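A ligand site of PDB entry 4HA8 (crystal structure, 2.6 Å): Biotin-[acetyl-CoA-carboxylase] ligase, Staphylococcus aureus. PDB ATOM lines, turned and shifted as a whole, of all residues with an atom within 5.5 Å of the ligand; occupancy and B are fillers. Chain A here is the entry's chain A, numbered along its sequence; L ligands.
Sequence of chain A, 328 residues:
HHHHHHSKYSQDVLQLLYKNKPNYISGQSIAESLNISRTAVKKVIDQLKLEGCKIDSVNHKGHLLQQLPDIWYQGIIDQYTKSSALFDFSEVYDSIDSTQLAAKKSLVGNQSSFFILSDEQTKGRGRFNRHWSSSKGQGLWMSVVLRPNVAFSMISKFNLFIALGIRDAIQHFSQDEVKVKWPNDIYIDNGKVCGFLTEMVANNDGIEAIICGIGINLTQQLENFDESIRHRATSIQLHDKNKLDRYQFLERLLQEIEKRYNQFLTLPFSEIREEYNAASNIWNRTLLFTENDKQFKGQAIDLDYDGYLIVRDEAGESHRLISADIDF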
ATOM      1  N   SER A  98       1.484  31.738  -4.238  1.00  0.00           N
ATOM      2  CA  SER A  98       0.881  30.890  -5.225  1.00  0.00           C
ATOM      3  C   SER A  98       0.662  31.647  -6.537  1.00  0.00           C
ATOM      4  O   SER A  98       0.118  32.779  -6.557  1.00  0.00           O
ATOM      5  CB  SER A  98      -0.458  30.408  -4.681  1.00  0.00           C
ATOM      6  OG  SER A  98      -1.292  30.011  -5.746  1.00  0.00           O
ATOM      7  N   THR A  99       1.037  31.018  -7.641  1.00  0.00           N
ATOM      8  CA  THR A  99       0.838  31.673  -8.933  1.00  0.00           C
ATOM      9  C   THR A  99      -0.654  31.882  -9.207  1.00  0.00           C
ATOM     10  O   THR A  99      -1.053  32.806  -9.900  1.00  0.00           O
ATOM     11  CB  THR A  99       1.439  30.898 -10.100  1.00  0.00           C
ATOM     12  OG1 THR A  99       0.757  29.644 -10.211  1.00  0.00           O
ATOM     13  CG2 THR A  99       2.943  30.674  -9.880  1.00  0.00           C
ATOM     14  N   GLN A 100      -1.469  31.019  -8.612  1.00  0.00           N
ATOM     15  CA  GLN A 100      -2.923  31.137  -8.729  1.00  0.00           C
ATOM     16  C   GLN A 100      -3.411  32.385  -8.012  1.00  0.00           C
ATOM     17  O   GLN A 100      -4.228  33.125  -8.550  1.00  0.00           O
ATOM     18  CB  GLN A 100      -3.589  29.850  -8.243  1.00  0.00           C
ATOM     19  CG  GLN A 100      -4.941  29.530  -8.840  1.00  0.00           C
ATOM     20  CD  GLN A 100      -4.986  29.147 -10.358  1.00  0.00           C
ATOM     21  OE1 GLN A 100      -6.061  28.946 -10.898  1.00  0.00           O
ATOM     22  NE2 GLN A 100      -3.859  29.077 -11.029  1.00  0.00           N
ATOM     23  N   GLN A 121       6.520  27.809  -4.687  1.00  0.00           N
ATOM     24  CA  GLN A 121       5.329  28.408  -4.058  1.00  0.00           C
ATOM     25  C   GLN A 121       5.309  28.020  -2.591  1.00  0.00           C
ATOM     26  O   GLN A 121       5.577  26.888  -2.229  1.00  0.00           O
ATOM     27  CB  GLN A 121       4.025  27.987  -4.746  1.00  0.00           C
ATOM     28  CG  GLN A 121       3.966  28.109  -6.277  1.00  0.00           C
ATOM     29  CD  GLN A 121       2.625  27.637  -6.838  1.00  0.00           C
ATOM     30  OE1 GLN A 121       1.846  28.401  -7.489  1.00  0.00           O
ATOM     31  NE2 GLN A 121       2.332  26.366  -6.609  1.00  0.00           N
ATOM     32  N   LYS A 123       2.615  28.554  -0.724  1.00  0.00           N
ATOM     33  CA  LYS A 123       1.236  28.165  -0.423  1.00  0.00           C
ATOM     34  C   LYS A 123       0.499  27.592  -1.629  1.00  0.00           C
ATOM     35  O   LYS A 123      -0.625  28.019  -1.986  1.00  0.00           O
ATOM     36  CB  LYS A 123       0.459  29.311   0.174  1.00  0.00           C
ATOM     37  CG  LYS A 123      -0.809  28.913   0.847  1.00  0.00           C
ATOM     38  CD  LYS A 123      -1.363  30.143   1.584  1.00  0.00           C
ATOM     39  CE  LYS A 123      -2.599  29.858   2.448  1.00  0.00           C
ATOM     40  NZ  LYS A 123      -2.643  30.992   3.419  1.00  0.00           N
ATOM     41  N   GLY A 124       1.142  26.623  -2.257  1.00  0.00           N
ATOM     42  CA  GLY A 124       0.520  26.043  -3.454  1.00  0.00           C
ATOM     43  C   GLY A 124      -0.712  25.223  -3.082  1.00  0.00           C
ATOM     44  O   GLY A 124      -0.684  24.445  -2.130  1.00  0.00           O
ATOM     45  N   ARG A 125      -1.781  25.420  -3.822  1.00  0.00           N
ATOM     46  CA  ARG A 125      -3.049  24.757  -3.556  1.00  0.00           C
ATOM     47  C   ARG A 125      -3.617  24.148  -4.810  1.00  0.00           C
ATOM     48  O   ARG A 125      -3.552  24.734  -5.897  1.00  0.00           O
ATOM     49  CB  ARG A 125      -4.036  25.762  -3.003  1.00  0.00           C
ATOM     50  CG  ARG A 125      -3.701  26.229  -1.585  1.00  0.00           C
ATOM     51  CD  ARG A 125      -3.616  25.112  -0.540  1.00  0.00           C
ATOM     52  NE  ARG A 125      -3.285  25.660   0.782  1.00  0.00           N
ATOM     53  CZ  ARG A 125      -2.029  25.714   1.267  1.00  0.00           C
ATOM     54  NH1 ARG A 125      -0.976  25.263   0.576  1.00  0.00           N
ATOM     55  NH2 ARG A 125      -1.816  26.229   2.461  1.00  0.00           N
ATOM     56  N   GLY A 126      -4.167  22.948  -4.665  1.00  0.00           N
ATOM     57  CA  GLY A 126      -4.957  22.338  -5.735  1.00  0.00           C
ATOM     58  C   GLY A 126      -6.448  22.435  -5.416  1.00  0.00           C
ATOM     59  O   GLY A 126      -6.931  23.398  -4.787  1.00  0.00           O
ATOM     60  N   ARG A 127      -7.199  21.439  -5.872  1.00  0.00           N
ATOM     61  CA  ARG A 127      -8.640  21.439  -5.707  1.00  0.00           C
ATOM     62  C   ARG A 127      -8.912  21.218  -4.274  1.00  0.00           C
ATOM     63  O   ARG A 127      -8.093  20.593  -3.574  1.00  0.00           O
ATOM     64  CB  ARG A 127      -9.249  20.326  -6.489  1.00  0.00           C
ATOM     65  CG  ARG A 127      -9.141  20.605  -7.973  1.00  0.00           C
ATOM     66  CD  ARG A 127      -9.492  19.455  -8.866  1.00  0.00           C
ATOM     67  NE  ARG A 127     -10.894  19.092  -8.726  1.00  0.00           N
ATOM     68  CZ  ARG A 127     -11.376  17.841  -8.845  1.00  0.00           C
ATOM     69  NH1 ARG A 127     -10.569  16.814  -9.067  1.00  0.00           N
ATOM     70  NH2 ARG A 127     -12.699  17.613  -8.699  1.00  0.00           N
ATOM     71  N   ARG A 130      -6.401  21.825  -1.260  1.00  0.00           N
ATOM     72  CA  ARG A 130      -5.410  20.869  -0.840  1.00  0.00           C
ATOM     73  C   ARG A 130      -3.994  21.342  -1.107  1.00  0.00           C
ATOM     74  O   ARG A 130      -3.672  22.002  -2.102  1.00  0.00           O
ATOM     75  CB  ARG A 130      -5.506  19.634  -1.675  1.00  0.00           C
ATOM     76  CG  ARG A 130      -6.494  18.653  -1.237  1.00  0.00           C
ATOM     77  CD  ARG A 130      -6.747  17.811  -2.414  1.00  0.00           C
ATOM     78  NE  ARG A 130      -7.814  16.910  -2.062  1.00  0.00           N
ATOM     79  CZ  ARG A 130      -8.608  16.302  -2.938  1.00  0.00           C
ATOM     80  NH1 ARG A 130      -8.403  16.487  -4.238  1.00  0.00           N
ATOM     81  NH2 ARG A 130      -9.569  15.515  -2.460  1.00  0.00           N
ATOM     82  N   HIS A 131      -3.098  20.911  -0.245  1.00  0.00           N
ATOM     83  CA  HIS A 131      -1.769  21.381  -0.311  1.00  0.00           C
ATOM     84  C   HIS A 131      -1.082  20.843  -1.570  1.00  0.00           C
ATOM     85  O   HIS A 131      -1.085  19.655  -1.817  1.00  0.00           O
ATOM     86  CB  HIS A 131      -1.059  21.012   0.968  1.00  0.00           C
ATOM     87  CG  HIS A 131       0.405  20.953   0.803  1.00  0.00           C
ATOM     88  ND1 HIS A 131       1.192  22.088   0.824  1.00  0.00           N
ATOM     89  CD2 HIS A 131       1.225  19.913   0.495  1.00  0.00           C
ATOM     90  CE1 HIS A 131       2.445  21.742   0.584  1.00  0.00           C
ATOM     91  NE2 HIS A 131       2.493  20.438   0.373  1.00  0.00           N
ATOM     92  N   TRP A 132      -0.492  21.690  -2.383  1.00  0.00           N
ATOM     93  CA  TRP A 132       0.338  21.190  -3.462  1.00  0.00           C
ATOM     94  C   TRP A 132       1.761  21.651  -3.204  1.00  0.00           C
ATOM     95  O   TRP A 132       2.053  22.838  -2.941  1.00  0.00           O
ATOM     96  CB  TRP A 132      -0.162  21.639  -4.843  1.00  0.00           C
ATOM     97  CG  TRP A 132       0.743  21.273  -5.961  1.00  0.00           C
ATOM     98  CD1 TRP A 132       1.635  22.112  -6.606  1.00  0.00           C
ATOM     99  CD2 TRP A 132       0.879  19.995  -6.602  1.00  0.00           C
ATOM    100  NE1 TRP A 132       2.334  21.415  -7.572  1.00  0.00           N
ATOM    101  CE2 TRP A 132       1.885  20.123  -7.607  1.00  0.00           C
ATOM    102  CE3 TRP A 132       0.265  18.751  -6.423  1.00  0.00           C
ATOM    103  CZ2 TRP A 132       2.275  19.034  -8.448  1.00  0.00           C
ATOM    104  CZ3 TRP A 132       0.662  17.667  -7.260  1.00  0.00           C
ATOM    105  CH2 TRP A 132       1.652  17.821  -8.251  1.00  0.00           C
ATOM    106  N   SER A 134       5.296  22.621  -4.017  1.00  0.00           N
ATOM    107  CA  SER A 134       5.882  23.343  -5.135  1.00  0.00           C
ATOM    108  C   SER A 134       7.358  23.705  -4.899  1.00  0.00           C
ATOM    109  O   SER A 134       7.744  24.853  -4.997  1.00  0.00           O
ATOM    110  CB  SER A 134       5.101  24.635  -5.370  1.00  0.00           C
ATOM    111  OG  SER A 134       3.722  24.444  -5.422  1.00  0.00           O
ATOM    112  N   LEU A 140       7.223  22.987 -12.720  1.00  0.00           N
ATOM    113  CA  LEU A 140       6.746  24.122 -13.419  1.00  0.00           C
ATOM    114  C   LEU A 140       5.508  24.449 -12.632  1.00  0.00           C
ATOM    115  O   LEU A 140       4.599  23.655 -12.571  1.00  0.00           O
ATOM    116  CB  LEU A 140       6.460  23.710 -14.808  1.00  0.00           C
ATOM    117  CG  LEU A 140       5.895  24.787 -15.677  1.00  0.00           C
ATOM    118  CD1 LEU A 140       6.356  24.522 -17.084  1.00  0.00           C
ATOM    119  CD2 LEU A 140       4.369  24.744 -15.633  1.00  0.00           C
ATOM    120  N   TRP A 141       5.501  25.600 -11.978  1.00  0.00           N
ATOM    121  CA  TRP A 141       4.331  26.028 -11.241  1.00  0.00           C
ATOM    122  C   TRP A 141       3.828  27.285 -11.902  1.00  0.00           C
ATOM    123  O   TRP A 141       4.417  28.363 -11.758  1.00  0.00           O
ATOM    124  CB  TRP A 141       4.651  26.281  -9.768  1.00  0.00           C
ATOM    125  CG  TRP A 141       5.686  25.358  -9.187  1.00  0.00           C
ATOM    126  CD1 TRP A 141       6.879  25.727  -8.631  1.00  0.00           C
ATOM    127  CD2 TRP A 141       5.657  23.925  -9.144  1.00  0.00           C
ATOM    128  NE1 TRP A 141       7.579  24.637  -8.191  1.00  0.00           N
ATOM    129  CE2 TRP A 141       6.870  23.512  -8.489  1.00  0.00           C
ATOM    130  CE3 TRP A 141       4.726  22.956  -9.515  1.00  0.00           C
ATOM    131  CZ2 TRP A 141       7.165  22.155  -8.215  1.00  0.00           C
ATOM    132  CZ3 TRP A 141       5.009  21.615  -9.272  1.00  0.00           C
ATOM    133  CH2 TRP A 141       6.222  21.215  -8.613  1.00  0.00           C
ATOM    134  N   MET A 142       2.735  27.141 -12.636  1.00  0.00           N
ATOM    135  CA  MET A 142       2.311  28.145 -13.550  1.00  0.00           C
ATOM    136  C   MET A 142       0.798  28.387 -13.401  1.00  0.00           C
ATOM    137  O   MET A 142       0.061  27.455 -13.061  1.00  0.00           O
ATOM    138  CB  MET A 142       2.610  27.671 -14.953  1.00  0.00           C
ATOM    139  CG  MET A 142       2.330  28.698 -15.993  1.00  0.00           C
ATOM    140  SD  MET A 142       2.907  28.184 -17.652  1.00  0.00           S
ATOM    141  CE  MET A 142       1.798  26.872 -17.985  1.00  0.00           C
ATOM    142  N   SER A 143       0.369  29.614 -13.662  1.00  0.00           N
ATOM    143  CA  SER A 143      -1.016  29.912 -13.796  1.00  0.00           C
ATOM    144  C   SER A 143      -1.210  30.691 -15.084  1.00  0.00           C
ATOM    145  O   SER A 143      -0.470  31.609 -15.351  1.00  0.00           O
ATOM    146  CB  SER A 143      -1.493  30.742 -12.633  1.00  0.00           C
ATOM    147  OG  SER A 143      -1.553  29.945 -11.452  1.00  0.00           O
ATOM    148  N   ASP A 185      -6.024  15.516 -13.521  1.00  0.00           N
ATOM    149  CA  ASP A 185      -4.688  15.061 -13.145  1.00  0.00           C
ATOM    150  C   ASP A 185      -4.027  14.284 -14.284  1.00  0.00           C
ATOM    151  O   ASP A 185      -4.730  13.782 -15.127  1.00  0.00           O
ATOM    152  CB  ASP A 185      -4.764  14.261 -11.873  1.00  0.00           C
ATOM    153  CG  ASP A 185      -5.167  15.114 -10.672  1.00  0.00           C
ATOM    154  OD1 ASP A 185      -6.382  15.228 -10.422  1.00  0.00           O
ATOM    155  OD2 ASP A 185      -4.273  15.641  -9.941  1.00  0.00           O
ATOM    156  N   LYS A 192       1.333  10.428 -10.331  1.00  0.00           N
ATOM    157  CA  LYS A 192       0.770  11.756 -10.720  1.00  0.00           C
ATOM    158  C   LYS A 192       1.961  12.659 -11.069  1.00  0.00           C
ATOM    159  O   LYS A 192       2.854  12.799 -10.296  1.00  0.00           O
ATOM    160  CB  LYS A 192      -0.106  12.360  -9.614  1.00  0.00           C
ATOM    161  CG  LYS A 192      -0.924  13.522 -10.110  1.00  0.00           C
ATOM    162  CD  LYS A 192      -1.343  14.486  -9.033  1.00  0.00           C
ATOM    163  CE  LYS A 192      -2.601  14.043  -8.359  1.00  0.00           C
ATOM    164  NZ  LYS A 192      -3.043  15.000  -7.280  1.00  0.00           N
ATOM    165  N   GLY A 195      -0.908  18.156 -11.736  1.00  0.00           N
ATOM    166  CA  GLY A 195      -2.267  18.498 -11.366  1.00  0.00           C
ATOM    167  C   GLY A 195      -2.590  19.820 -12.044  1.00  0.00           C
ATOM    168  O   GLY A 195      -1.741  20.657 -12.196  1.00  0.00           O
ATOM    169  N   PHE A 196      -3.806  20.009 -12.462  1.00  0.00           N
ATOM    170  CA  PHE A 196      -4.203  21.324 -12.905  1.00  0.00           C
ATOM    171  C   PHE A 196      -5.617  21.614 -12.424  1.00  0.00           C
ATOM    172  O   PHE A 196      -6.324  20.756 -11.938  1.00  0.00           O
ATOM    173  CB  PHE A 196      -4.096  21.457 -14.418  1.00  0.00           C
ATOM    174  CG  PHE A 196      -4.918  20.476 -15.170  1.00  0.00           C
ATOM    175  CD1 PHE A 196      -4.454  19.178 -15.403  1.00  0.00           C
ATOM    176  CD2 PHE A 196      -6.193  20.828 -15.634  1.00  0.00           C
ATOM    177  CE1 PHE A 196      -5.212  18.236 -16.072  1.00  0.00           C
ATOM    178  CE2 PHE A 196      -6.954  19.886 -16.347  1.00  0.00           C
ATOM    179  CZ  PHE A 196      -6.455  18.604 -16.566  1.00  0.00           C
ATOM    180  N   LEU A 197      -6.024  22.858 -12.621  1.00  0.00           N
ATOM    181  CA  LEU A 197      -7.183  23.365 -11.955  1.00  0.00           C
ATOM    182  C   LEU A 197      -7.626  24.509 -12.846  1.00  0.00           C
ATOM    183  O   LEU A 197      -6.836  25.430 -13.077  1.00  0.00           O
ATOM    184  CB  LEU A 197      -6.660  23.879 -10.621  1.00  0.00           C
ATOM    185  CG  LEU A 197      -7.471  24.732  -9.696  1.00  0.00           C
ATOM    186  CD1 LEU A 197      -8.690  23.961  -9.264  1.00  0.00           C
ATOM    187  CD2 LEU A 197      -6.626  25.042  -8.512  1.00  0.00           C
ATOM    188  N   GLY A 213      -4.463  26.974 -13.324  1.00  0.00           N
ATOM    189  CA  GLY A 213      -3.249  26.625 -12.587  1.00  0.00           C
ATOM    190  C   GLY A 213      -2.821  25.221 -12.956  1.00  0.00           C
ATOM    191  O   GLY A 213      -3.644  24.291 -12.919  1.00  0.00           O
ATOM    192  N   ILE A 214      -1.546  25.071 -13.317  1.00  0.00           N
ATOM    193  CA  ILE A 214      -0.918  23.844 -13.818  1.00  0.00           C
ATOM    194  C   ILE A 214       0.339  23.584 -13.011  1.00  0.00           C
ATOM    195  O   ILE A 214       1.212  24.434 -12.959  1.00  0.00           O
ATOM    196  CB  ILE A 214      -0.473  24.055 -15.215  1.00  0.00           C
ATOM    197  CG1 ILE A 214      -1.655  24.437 -16.096  1.00  0.00           C
ATOM    198  CG2 ILE A 214       0.197  22.829 -15.800  1.00  0.00           C
ATOM    199  CD1 ILE A 214      -1.215  24.764 -17.537  1.00  0.00           C
ATOM    200  N   GLY A 215       0.433  22.435 -12.337  1.00  0.00           N
ATOM    201  CA  GLY A 215       1.624  22.093 -11.594  1.00  0.00           C
ATOM    202  C   GLY A 215       2.182  20.794 -12.144  1.00  0.00           C
ATOM    203  O   GLY A 215       1.473  19.768 -12.221  1.00  0.00           O
HETATM  204  C1  LIG L   1      -3.162  19.153  -5.379  1.00  0.00           C
HETATM  205  C2  LIG L   1      -2.885  19.475  -6.523  1.00  0.00           C
HETATM  206  C3  LIG L   1      -2.435  19.928  -7.916  1.00  0.00           C
HETATM  207  C4  LIG L   1      -3.064  21.294  -8.378  1.00  0.00           C
HETATM  208  C5  LIG L   1      -2.205  22.207  -9.301  1.00  0.00           C
HETATM  209  C6  LIG L   1      -1.378  23.273  -8.589  1.00  0.00           C
HETATM  210  C7  LIG L   1      -0.928  24.350  -9.592  1.00  0.00           C
HETATM  211  S1  LIG L   1       0.776  24.838  -9.214  1.00  0.00           S
HETATM  212  C8  LIG L   1       0.638  26.443  -9.977  1.00  0.00           C
HETATM  213  C9  LIG L   1      -0.760  26.869  -9.562  1.00  0.00           C
HETATM  214  C10 LIG L   1      -1.660  25.651  -9.283  1.00  0.00           C
HETATM  215  N1  LIG L   1      -1.958  25.739  -7.847  1.00  0.00           N
HETATM  216  C11 LIG L   1      -1.356  26.816  -7.345  1.00  0.00           C
HETATM  217  O1  LIG L   1      -1.402  27.158  -6.155  1.00  0.00           O
HETATM  218  N2  LIG L   1      -0.636  27.474  -8.261  1.00  0.00           N
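A sulfur (S1) of the ligand lies close to the backbone carbonyl oxygen (O) of Ile 214. N of Gln 100 touches N2 of the ligand, at 3.7 Å. CA of Gly 124 touches O1 of the ligand (3.5 Å). CA of Gly 126 touches C4 of the ligand, at 3.4 Å. CE3 of Trp 132 touches C2 of the ligand, 3.2 Å away. Trp 141 touches the ligand. Met 142 touches the ligand (O to C8, 3.3 Å). Ser 143 touches the ligand (OG to C9, 3.7 Å). Gly 195 touches the ligand. Gly 213 touches the ligand (CA to C10, 3.8 Å). N of Gly 215 touches C7 of the ligand, at 3.6 Å. 15 residues have an atom within 4 Å of the ligand: Ser 98, Thr 99, Gln 100, Gln 121, Gly 124, Arg 125, Gly 126, Trp 132, Trp 141, Met 142, Ser 143, Gly 195, Gly 213, Ile 214 and Gly 215.
A nitrogen (N1) of the ligand lies within hydrogen-bond range of the backbone carbonyl oxygen of Arg 125 (2.7 Å). An oxygen (O1) of the ligand sits at hydrogen-bond distance from the backbone NH (N) of Arg 125, 2.9 Å away. OG1 of Thr 99 sits close to N2 of the ligand. The side-chain hydroxyl of Ser 98 is in hydrogen-bond range of an oxygen (O1) of the ligand, at 2.9 Å. The side-chain amide oxygen of Gln 121 is in hydrogen-bond range of a nitrogen (N2) of the ligand, 2.8 Å away.
The backbone NH (N) of Trp 132 sits at hydrogen-bond distance from the backbone carbonyl oxygen (O) of Gly 124 (2.8 Å). The backbone NH (N) of Gly 215 lies within hydrogen-bond range of the backbone carbonyl oxygen (O) of Gly 195 (2.8 Å). The backbone carbonyl oxygen (O) of Trp 132 lies close to the side-chain hydroxyl (OG) of Ser 134, at 3.4 Å. The backbone NH (N) of Leu 197 lies within hydrogen-bond range of the backbone carbonyl oxygen (O) of Gly 213, 2.8 Å away. OG of Ser 134 sits at hydrogen-bond distance from NE2 of Gln 121. NE2 of Gln 100 lies close to N of Gly 213. The side-chain hydroxyl of Thr 99 is in hydrogen-bond range of the side-chain hydroxyl of Ser 143 (2.6 Å). The indole nitrogen (NE1) of Trp 141 is in hydrogen-bond range of the backbone carbonyl oxygen (O) of Ser 134, 3.2 Å away.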
